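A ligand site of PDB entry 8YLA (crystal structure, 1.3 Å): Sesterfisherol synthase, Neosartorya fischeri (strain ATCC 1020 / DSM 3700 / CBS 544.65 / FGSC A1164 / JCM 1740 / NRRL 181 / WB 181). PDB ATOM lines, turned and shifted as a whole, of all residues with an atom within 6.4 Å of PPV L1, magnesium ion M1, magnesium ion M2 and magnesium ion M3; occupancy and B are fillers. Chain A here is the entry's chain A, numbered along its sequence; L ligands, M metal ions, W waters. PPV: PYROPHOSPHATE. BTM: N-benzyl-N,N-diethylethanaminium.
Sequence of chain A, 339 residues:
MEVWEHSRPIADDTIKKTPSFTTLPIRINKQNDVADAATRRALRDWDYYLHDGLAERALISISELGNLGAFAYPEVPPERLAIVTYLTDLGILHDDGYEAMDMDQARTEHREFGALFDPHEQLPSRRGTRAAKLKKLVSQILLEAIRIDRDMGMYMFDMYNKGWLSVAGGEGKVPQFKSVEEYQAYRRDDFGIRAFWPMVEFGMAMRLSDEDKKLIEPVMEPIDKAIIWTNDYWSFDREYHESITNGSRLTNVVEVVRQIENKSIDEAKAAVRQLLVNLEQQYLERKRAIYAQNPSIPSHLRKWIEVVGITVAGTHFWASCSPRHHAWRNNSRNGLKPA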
ATOM      1  N   ILE A  92     -32.525   8.985   6.743  1.00  0.00           N
ATOM      2  CA  ILE A  92     -31.557   9.907   7.355  1.00  0.00           C
ATOM      3  C   ILE A  92     -31.773  11.324   6.844  1.00  0.00           C
ATOM      4  O   ILE A  92     -31.780  12.277   7.619  1.00  0.00           O
ATOM      5  CB  ILE A  92     -30.113   9.444   7.091  1.00  0.00           C
ATOM      6  CG1 ILE A  92     -29.834   8.098   7.775  1.00  0.00           C
ATOM      7  CG2 ILE A  92     -29.127  10.499   7.577  1.00  0.00           C
ATOM      8  CD1 ILE A  92     -28.531   7.447   7.322  1.00  0.00           C
ATOM      9  N   ASP A  95     -34.835  12.659   8.334  1.00  0.00           N
ATOM     10  CA  ASP A  95     -34.658  12.911   9.766  1.00  0.00           C
ATOM     11  C   ASP A  95     -33.815  14.141  10.016  1.00  0.00           C
ATOM     12  O   ASP A  95     -34.059  14.867  10.992  1.00  0.00           O
ATOM     13  CB  ASP A  95     -34.042  11.691  10.460  1.00  0.00           C
ATOM     14  CG  ASP A  95     -34.187  11.783  11.970  1.00  0.00           C
ATOM     15  OD1 ASP A  95     -35.339  11.863  12.449  1.00  0.00           O
ATOM     16  OD2 ASP A  95     -33.142  11.783  12.670  1.00  0.00           O
ATOM     17  N   ASP A  96     -32.845  14.403   9.147  1.00  0.00           N
ATOM     18  CA  ASP A  96     -32.056  15.624   9.291  1.00  0.00           C
ATOM     19  C   ASP A  96     -32.947  16.865   9.130  1.00  0.00           C
ATOM     20  O   ASP A  96     -32.792  17.844   9.857  1.00  0.00           O
ATOM     21  CB  ASP A  96     -30.898  15.641   8.297  1.00  0.00           C
ATOM     22  CG  ASP A  96     -29.740  14.763   8.739  1.00  0.00           C
ATOM     23  OD1 ASP A  96     -29.786  14.205   9.866  1.00  0.00           O
ATOM     24  OD2 ASP A  96     -28.797  14.603   7.936  1.00  0.00           O
ATOM     25  N   TYR A  98     -36.217  16.902   9.781  1.00  0.00           N
ATOM     26  CA  TYR A  98     -37.039  16.870  10.990  1.00  0.00           C
ATOM     27  C   TYR A  98     -36.322  17.514  12.169  1.00  0.00           C
ATOM     28  O   TYR A  98     -36.914  18.294  12.910  1.00  0.00           O
ATOM     29  CB  TYR A  98     -37.394  15.409  11.275  1.00  0.00           C
ATOM     30  CG  TYR A  98     -37.937  15.080  12.639  1.00  0.00           C
ATOM     31  CD1 TYR A  98     -39.307  15.112  12.883  1.00  0.00           C
ATOM     32  CD2 TYR A  98     -37.087  14.668  13.661  1.00  0.00           C
ATOM     33  CE1 TYR A  98     -39.811  14.778  14.123  1.00  0.00           C
ATOM     34  CE2 TYR A  98     -37.597  14.336  14.909  1.00  0.00           C
ATOM     35  CZ  TYR A  98     -38.962  14.383  15.127  1.00  0.00           C
ATOM     36  OH  TYR A  98     -39.494  14.036  16.349  1.00  0.00           O
ATOM     37  N   GLU A  99     -35.059  17.154  12.358  1.00  0.00           N
ATOM     38  CA  GLU A  99     -34.274  17.666  13.482  1.00  0.00           C
ATOM     39  C   GLU A  99     -34.047  19.177  13.434  1.00  0.00           C
ATOM     40  O   GLU A  99     -33.829  19.808  14.460  1.00  0.00           O
ATOM     41  CB  GLU A  99     -32.914  16.945  13.559  1.00  0.00           C
ATOM     42  CG  GLU A  99     -33.018  15.488  13.974  1.00  0.00           C
ATOM     43  CD  GLU A  99     -31.702  14.941  14.489  1.00  0.00           C
ATOM     44  OE1 GLU A  99     -30.980  15.672  15.193  1.00  0.00           O
ATOM     45  OE2 GLU A  99     -31.390  13.764  14.180  1.00  0.00           O
ATOM     46  N   ARG A 187     -36.028   7.455  23.025  1.00  0.00           N
ATOM     47  CA  ARG A 187     -35.014   7.260  21.989  1.00  0.00           C
ATOM     48  C   ARG A 187     -35.351   6.060  21.114  1.00  0.00           C
ATOM     49  O   ARG A 187     -35.072   6.079  19.913  1.00  0.00           O
ATOM     50  CB  ARG A 187     -33.624   7.142  22.614  1.00  0.00           C
ATOM     51  CG  ARG A 187     -32.520   7.000  21.608  1.00  0.00           C
ATOM     52  CD  ARG A 187     -32.346   8.238  20.723  1.00  0.00           C
ATOM     53  NE  ARG A 187     -31.068   8.175  20.039  1.00  0.00           N
ATOM     54  CZ  ARG A 187     -30.874   8.281  18.734  1.00  0.00           C
ATOM     55  NH1 ARG A 187     -31.848   8.614  17.909  1.00  0.00           N
ATOM     56  NH2 ARG A 187     -29.660   8.037  18.244  1.00  0.00           N
ATOM     57  N   ASP A 190     -37.528   7.616  18.591  1.00  0.00           N
ATOM     58  CA  ASP A 190     -36.842   8.607  17.770  1.00  0.00           C
ATOM     59  C   ASP A 190     -35.821   7.966  16.847  1.00  0.00           C
ATOM     60  O   ASP A 190     -35.578   8.458  15.736  1.00  0.00           O
ATOM     61  CB  ASP A 190     -36.167   9.621  18.699  1.00  0.00           C
ATOM     62  CG  ASP A 190     -35.268  10.585  17.948  1.00  0.00           C
ATOM     63  OD1 ASP A 190     -35.801  11.455  17.232  1.00  0.00           O
ATOM     64  OD2 ASP A 190     -34.033  10.471  18.076  1.00  0.00           O
ATOM     65  N   PHE A 191     -35.183   6.874  17.289  1.00  0.00           N
ATOM     66  CA  PHE A 191     -34.238   6.120  16.466  1.00  0.00           C
ATOM     67  C   PHE A 191     -34.942   5.236  15.453  1.00  0.00           C
ATOM     68  O   PHE A 191     -34.330   4.847  14.454  1.00  0.00           O
ATOM     69  CB  PHE A 191     -33.398   5.219  17.392  1.00  0.00           C
ATOM     70  CG  PHE A 191     -32.266   4.496  16.720  1.00  0.00           C
ATOM     71  CD1 PHE A 191     -31.001   5.071  16.658  1.00  0.00           C
ATOM     72  CD2 PHE A 191     -32.431   3.204  16.212  1.00  0.00           C
ATOM     73  CE1 PHE A 191     -29.936   4.395  16.077  1.00  0.00           C
ATOM     74  CE2 PHE A 191     -31.367   2.532  15.617  1.00  0.00           C
ATOM     75  CZ  PHE A 191     -30.125   3.122  15.559  1.00  0.00           C
ATOM     76  N   ILE A 228     -28.199   1.701  19.615  1.00  0.00           N
ATOM     77  CA  ILE A 228     -28.650   3.079  19.760  1.00  0.00           C
ATOM     78  C   ILE A 228     -27.584   3.917  20.433  1.00  0.00           C
ATOM     79  O   ILE A 228     -27.232   5.009  19.959  1.00  0.00           O
ATOM     80  CB  ILE A 228     -29.982   3.110  20.514  1.00  0.00           C
ATOM     81  CG1 ILE A 228     -31.066   2.439  19.679  1.00  0.00           C
ATOM     82  CG2 ILE A 228     -30.348   4.530  20.884  1.00  0.00           C
ATOM     83  CD1 ILE A 228     -32.375   2.276  20.400  1.00  0.00           C
ATOM     84  N   ASN A 231     -24.560   4.845  18.212  1.00  0.00           N
ATOM     85  CA  ASN A 231     -24.783   6.070  17.462  1.00  0.00           C
ATOM     86  C   ASN A 231     -24.649   7.276  18.370  1.00  0.00           C
ATOM     87  O   ASN A 231     -24.026   8.267  17.993  1.00  0.00           O
ATOM     88  CB  ASN A 231     -26.128   6.093  16.754  1.00  0.00           C
ATOM     89  CG  ASN A 231     -26.398   7.457  16.162  1.00  0.00           C
ATOM     90  OD1 ASN A 231     -26.984   8.317  16.822  1.00  0.00           O
ATOM     91  ND2 ASN A 231     -25.904   7.704  14.951  1.00  0.00           N
ATOM     92  N   ASP A 232     -25.251   7.221  19.563  1.00  0.00           N
ATOM     93  CA  ASP A 232     -25.202   8.408  20.436  1.00  0.00           C
ATOM     94  C   ASP A 232     -23.751   8.785  20.729  1.00  0.00           C
ATOM     95  O   ASP A 232     -23.384   9.964  20.672  1.00  0.00           O
ATOM     96  CB  ASP A 232     -25.912   8.130  21.759  1.00  0.00           C
ATOM     97  CG  ASP A 232     -27.434   8.099  21.655  1.00  0.00           C
ATOM     98  OD1 ASP A 232     -28.019   8.405  20.582  1.00  0.00           O
ATOM     99  OD2 ASP A 232     -28.048   7.768  22.704  1.00  0.00           O
ATOM    100  N   SER A 235     -22.122  10.362  17.580  1.00  0.00           N
ATOM    101  CA  SER A 235     -22.799  11.535  17.033  1.00  0.00           C
ATOM    102  C   SER A 235     -22.961  12.669  18.042  1.00  0.00           C
ATOM    103  O   SER A 235     -23.507  13.713  17.684  1.00  0.00           O
ATOM    104  CB  SER A 235     -24.143  11.168  16.380  1.00  0.00           C
ATOM    105  OG  SER A 235     -25.079  10.620  17.302  1.00  0.00           O
ATOM    106  N   PHE A 236     -22.464  12.507  19.266  1.00  0.00           N
ATOM    107  CA  PHE A 236     -22.647  13.540  20.285  1.00  0.00           C
ATOM    108  C   PHE A 236     -22.088  14.893  19.838  1.00  0.00           C
ATOM    109  O   PHE A 236     -22.757  15.923  19.984  1.00  0.00           O
ATOM    110  CB  PHE A 236     -22.025  13.139  21.618  1.00  0.00           C
ATOM    111  CG  PHE A 236     -22.065  14.249  22.637  1.00  0.00           C
ATOM    112  CD1 PHE A 236     -23.194  14.470  23.408  1.00  0.00           C
ATOM    113  CD2 PHE A 236     -20.975  15.103  22.818  1.00  0.00           C
ATOM    114  CE1 PHE A 236     -23.247  15.502  24.334  1.00  0.00           C
ATOM    115  CE2 PHE A 236     -21.017  16.140  23.739  1.00  0.00           C
ATOM    116  CZ  PHE A 236     -22.151  16.340  24.511  1.00  0.00           C
ATOM    117  N   ARG A 238     -21.587  16.410  16.979  1.00  0.00           N
ATOM    118  CA  ARG A 238     -22.426  17.113  16.003  1.00  0.00           C
ATOM    119  C   ARG A 238     -23.735  17.545  16.641  1.00  0.00           C
ATOM    120  O   ARG A 238     -24.190  18.680  16.447  1.00  0.00           O
ATOM    121  CB  ARG A 238     -22.704  16.225  14.793  1.00  0.00           C
ATOM    122  CG  ARG A 238     -23.894  16.704  13.928  1.00  0.00           C
ATOM    123  CD  ARG A 238     -23.999  15.959  12.619  1.00  0.00           C
ATOM    124  NE  ARG A 238     -23.936  14.516  12.785  1.00  0.00           N
ATOM    125  CZ  ARG A 238     -24.924  13.741  13.247  1.00  0.00           C
ATOM    126  NH1 ARG A 238     -26.078  14.255  13.646  1.00  0.00           N
ATOM    127  NH2 ARG A 238     -24.728  12.433  13.311  1.00  0.00           N
ATOM    128  N   GLU A 239     -24.375  16.645  17.370  1.00  0.00           N
ATOM    129  CA  GLU A 239     -25.679  16.931  17.935  1.00  0.00           C
ATOM    130  C   GLU A 239     -25.599  18.019  19.002  1.00  0.00           C
ATOM    131  O   GLU A 239     -26.493  18.873  19.085  1.00  0.00           O
ATOM    132  CB  GLU A 239     -26.299  15.633  18.474  1.00  0.00           C
ATOM    133  CG  GLU A 239     -26.629  14.699  17.339  1.00  0.00           C
ATOM    134  CD  GLU A 239     -26.984  13.296  17.777  1.00  0.00           C
ATOM    135  OE1 GLU A 239     -26.975  13.033  19.010  1.00  0.00           O
ATOM    136  OE2 GLU A 239     -27.282  12.477  16.869  1.00  0.00           O
ATOM    137  N   THR A 251     -30.837  14.774  21.594  1.00  0.00           N
ATOM    138  CA  THR A 251     -31.371  13.454  21.948  1.00  0.00           C
ATOM    139  C   THR A 251     -30.176  12.499  21.933  1.00  0.00           C
ATOM    140  O   THR A 251     -29.830  11.928  20.904  1.00  0.00           O
ATOM    141  CB  THR A 251     -32.456  13.022  20.969  1.00  0.00           C
ATOM    142  OG1 THR A 251     -33.407  14.090  20.821  1.00  0.00           O
ATOM    143  CG2 THR A 251     -33.152  11.783  21.486  1.00  0.00           C
ATOM    144  N   ASN A 252     -29.537  12.320  23.090  1.00  0.00           N
ATOM    145  CA  ASN A 252     -28.274  11.605  23.115  1.00  0.00           C
ATOM    146  C   ASN A 252     -27.977  11.167  24.542  1.00  0.00           C
ATOM    147  O   ASN A 252     -28.003  11.996  25.454  1.00  0.00           O
ATOM    148  CB  ASN A 252     -27.172  12.535  22.572  1.00  0.00           C
ATOM    149  CG  ASN A 252     -25.894  11.802  22.301  1.00  0.00           C
ATOM    150  OD1 ASN A 252     -25.326  11.192  23.208  1.00  0.00           O
ATOM    151  ND2 ASN A 252     -25.425  11.846  21.074  1.00  0.00           N
ATOM    152  N   TRP A 318     -18.200   1.913  11.258  1.00  0.00           N
ATOM    153  CA  TRP A 318     -18.501   2.991  10.330  1.00  0.00           C
ATOM    154  C   TRP A 318     -18.551   4.338  11.044  1.00  0.00           C
ATOM    155  O   TRP A 318     -17.984   5.326  10.585  1.00  0.00           O
ATOM    156  CB  TRP A 318     -19.822   2.698   9.623  1.00  0.00           C
ATOM    157  CG  TRP A 318     -20.189   3.721   8.606  1.00  0.00           C
ATOM    158  CD1 TRP A 318     -19.837   3.708   7.289  1.00  0.00           C
ATOM    159  CD2 TRP A 318     -20.950   4.925   8.803  1.00  0.00           C
ATOM    160  NE1 TRP A 318     -20.331   4.829   6.652  1.00  0.00           N
ATOM    161  CE2 TRP A 318     -21.013   5.589   7.562  1.00  0.00           C
ATOM    162  CE3 TRP A 318     -21.587   5.500   9.915  1.00  0.00           C
ATOM    163  CZ2 TRP A 318     -21.707   6.795   7.396  1.00  0.00           C
ATOM    164  CZ3 TRP A 318     -22.280   6.710   9.734  1.00  0.00           C
ATOM    165  CH2 TRP A 318     -22.325   7.336   8.492  1.00  0.00           C
ATOM    166  N   ARG A 324     -20.199  12.054   8.533  1.00  0.00           N
ATOM    167  CA  ARG A 324     -21.389  12.634   9.146  1.00  0.00           C
ATOM    168  C   ARG A 324     -21.170  13.011  10.604  1.00  0.00           C
ATOM    169  O   ARG A 324     -21.512  14.116  11.025  1.00  0.00           O
ATOM    170  CB  ARG A 324     -22.565  11.662   9.020  1.00  0.00           C
ATOM    171  CG  ARG A 324     -23.830  12.120   9.724  1.00  0.00           C
ATOM    172  CD  ARG A 324     -24.997  11.191   9.413  1.00  0.00           C
ATOM    173  NE  ARG A 324     -26.203  11.577  10.144  1.00  0.00           N
ATOM    174  CZ  ARG A 324     -27.177  12.322   9.635  1.00  0.00           C
ATOM    175  NH1 ARG A 324     -27.092  12.783   8.397  1.00  0.00           N
ATOM    176  NH2 ARG A 324     -28.237  12.617  10.375  1.00  0.00           N
ATOM    177  N   HIS A 325     -20.370  12.163  11.250  1.00  0.00           N
ATOM    178  CA  HIS A 325     -20.123  12.365  12.686  1.00  0.00           C
ATOM    179  C   HIS A 325     -18.861  13.100  13.059  1.00  0.00           C
ATOM    180  O   HIS A 325     -18.703  13.642  14.062  1.00  0.00           O
ATOM    181  CB  HIS A 325     -20.089  11.006  13.443  1.00  0.00           C
ATOM    182  CG  HIS A 325     -21.283  10.140  13.249  1.00  0.00           C
ATOM    183  ND1 HIS A 325     -22.561  10.623  13.105  1.00  0.00           N
ATOM    184  CD2 HIS A 325     -21.384   8.797  13.233  1.00  0.00           C
ATOM    185  CE1 HIS A 325     -23.384   9.606  12.983  1.00  0.00           C
ATOM    186  NE2 HIS A 325     -22.708   8.482  13.075  1.00  0.00           N
HETATM  187  O11 PPV L   1     -30.847   8.811  15.213  1.00  0.00           O
HETATM  188  P1  PPV L   1     -29.956  10.003  15.017  1.00  0.00           P
HETATM  189  O21 PPV L   1     -29.170  10.349  16.252  1.00  0.00           O
HETATM  190  O31 PPV L   1     -30.714  11.182  14.470  1.00  0.00           O
HETATM  191  OPP PPV L   1     -28.883   9.610  13.873  1.00  0.00           O
HETATM  192  P2  PPV L   1     -27.571  10.496  13.505  1.00  0.00           P
HETATM  193  O12 PPV L   1     -26.896   9.807  12.350  1.00  0.00           O
HETATM  194  O22 PPV L   1     -28.079  11.877  13.138  1.00  0.00           O
HETATM  195  O32 PPV L   1     -26.673  10.535  14.715  1.00  0.00           O
HETATM  196  N   BTM L   2     -32.368   6.532  11.303  1.00  0.00           N
HETATM  197  C1  BTM L   2     -32.687   6.098   9.938  1.00  0.00           C
HETATM  198  C2  BTM L   2     -33.373   7.512  11.759  1.00  0.00           C
HETATM  199  C3  BTM L   2     -34.589   6.779  12.277  1.00  0.00           C
HETATM  200  C4  BTM L   2     -32.360   5.376  12.205  1.00  0.00           C
HETATM  201  C5  BTM L   2     -31.197   4.471  11.852  1.00  0.00           C
HETATM  202  C6  BTM L   2     -31.037   7.170  11.303  1.00  0.00           C
HETATM  203  C7  BTM L   2     -30.496   7.188  12.719  1.00  0.00           C
HETATM  204  C8  BTM L   2     -33.732   5.001   9.988  1.00  0.00           C
HETATM  205  C9  BTM L   2     -33.336   3.682  10.134  1.00  0.00           C
HETATM  206  C10 BTM L   2     -34.290   2.663  10.169  1.00  0.00           C
HETATM  207  C11 BTM L   2     -35.640   2.987  10.064  1.00  0.00           C
HETATM  208  C12 BTM L   2     -36.037   4.307   9.917  1.00  0.00           C
HETATM  209  C13 BTM L   2     -35.082   5.315   9.873  1.00  0.00           C
HETATM  210 MG    MG M   1     -32.665  11.875  14.666  1.00  0.00          MG
HETATM  211 MG    MG M   2     -29.798  12.860  13.515  1.00  0.00          MG
HETATM  212 MG    MG M   3     -27.191  10.446  16.696  1.00  0.00          MG
HETATM  213  O   HOH W   1     -27.607  10.406  18.743  1.00  0.00           O
HETATM  214  O   HOH W   2     -30.202  12.191  18.102  1.00  0.00           O
HETATM  215  O   HOH W   3     -28.954  13.736  15.171  1.00  0.00           O
HETATM  216  O   HOH W   4     -29.340  14.644  12.549  1.00  0.00           O
HETATM  217  O   HOH W   5     -34.596  12.590  15.013  1.00  0.00           O
HETATM  218  O   HOH W   6     -32.523  12.163  16.749  1.00  0.00           O
HETATM  219  O   HOH W   7     -33.278   9.887  14.891  1.00  0.00           O
HETATM  220  O   HOH W   8     -30.727  12.340  11.722  1.00  0.00           O
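Magnesium ion M3 is bound by O21 of PPV L1 (2.0 Å), OE2 of Glu 239 (2.0 Å), O32 of PPV L1 (2.0 Å), water W1 (2.1 Å), OD1 of Asn 231 (2.1 Å) and OG of Ser 235 (2.2 Å). Magnesium ion M3 has six donor atoms within binding distance.
NH2 of Arg 187 lies within salt-bridge range of OD1 of Asp 232, at 2.9 Å. ND1 of His 325 sits at hydrogen-bond distance from NH2 of Arg 238 (2.8 Å). The backbone carbonyl oxygen (O) of Arg 324 is in hydrogen-bond range of the guanidinium group (NE) of Arg 238 (3.0 Å). The side-chain amide oxygen (OD1) of Asn 231 lies close to the guanidinium group (NH2) of Arg 187 (3.0 Å). OD2 of Asp 96 lies within salt-bridge range of NH1 of Arg 324 (2.5 Å). The guanidinium group (NH1) of Arg 238 sits close to the side-chain carboxylate (OE2) of Glu 239 (3.9 Å). The guanidinium group (NH1) of Arg 187 lies within salt-bridge range of the side-chain carboxylate (OD2) of Asp 190 (2.9 Å). ND2 of Asn 252 sits at hydrogen-bond distance from OE1 of Glu 239 (2.8 Å).
Magnesium ion M1 is bound by OD2 of Asp 95 (2.1 Å), O31 of PPV L1 (2.1 Å), water W5 (2.1 Å), water W7 (2.1 Å), water W6 (2.1 Å) and OE2 of Glu 99 (2.3 Å). Magnesium ion M1 has six donor atoms within binding distance.
Residues that only touch magnesium ion M3: Arg 187 (3.8 Å).
Water W5 bridges OD1 of Asp 95 and OD1 of Asp 190. Water W7 lies within hydrogen-bond range of an oxygen (O11) of PPV L1 (2.7 Å) and the backbone carbonyl oxygen (O) of Asp 190 (2.8 Å). Water W8 bridges the side-chain carboxylate (OD1) of Asp 96 (2.8 Å) and the guanidinium group (NH2) of Arg 324 (2.8 Å). Water W4 lies within hydrogen-bond range of OD1 of Asp 96 (2.8 Å), NH2 of Arg 324 (3.2 Å), OE1 of Glu 99 (3.3 Å) and NH1 of Arg 238 (3.5 Å). Water W3 lies within hydrogen-bond range of OE1 of Glu 99 (2.8 Å) and NH1 of Arg 238 (3.3 Å). Water W2 bridges O of Thr 251 and OE1 of Glu 239.
Merely in contact with magnesium ion M2: Asp 96 (3.9 Å), Arg 238 (3.98 Å) and Arg 324 (3.5 Å). The nearest printed residue that does not touch magnesium ion M2 is Glu 239 (4.2 Å).
His 325 touches PPV L1. Hydrophobic or aromatic side chains within 4 Å of PPV L1: His 325. Nine residues have an atom within 4 Å of PPV L1: Asp 95, Glu 99, Arg 187, Asn 231, Ser 235, Arg 238, Glu 239, Arg 324 and His 325. Along chain A the residues within 4 Å of PPV L1 span positions 95 to 325.
The guanidinium group (NH1) of Arg 187 is in salt-bridge range of an oxygen (O11) of PPV L1, at 2.9 Å. The guanidinium group of Arg 324 lies within salt-bridge range of an oxygen (O12) of PPV L1 (2.9 Å). The guanidinium group (NH2) of Arg 238 lies within salt-bridge range of an oxygen (O12) of PPV L1.
OE2 of Glu 99 binds magnesium ion M2, at 1.9 Å. O22 of PPV L1 is bound to magnesium ion M2 (2.0 Å). Water W3 is bound to magnesium ion M2 (2.1 Å). Water W4 is bound to magnesium ion M2. Magnesium ion M2 is bound by water W8 (2.1 Å). Magnesium ion M2 is bound by an oxygen (O31) of PPV L1, at 2.1 Å.
Asp 190 touches magnesium ion M1. Three residues have an atom within 4 Å of magnesium ion M1: Asp 95, Glu 99 and Asp 190.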
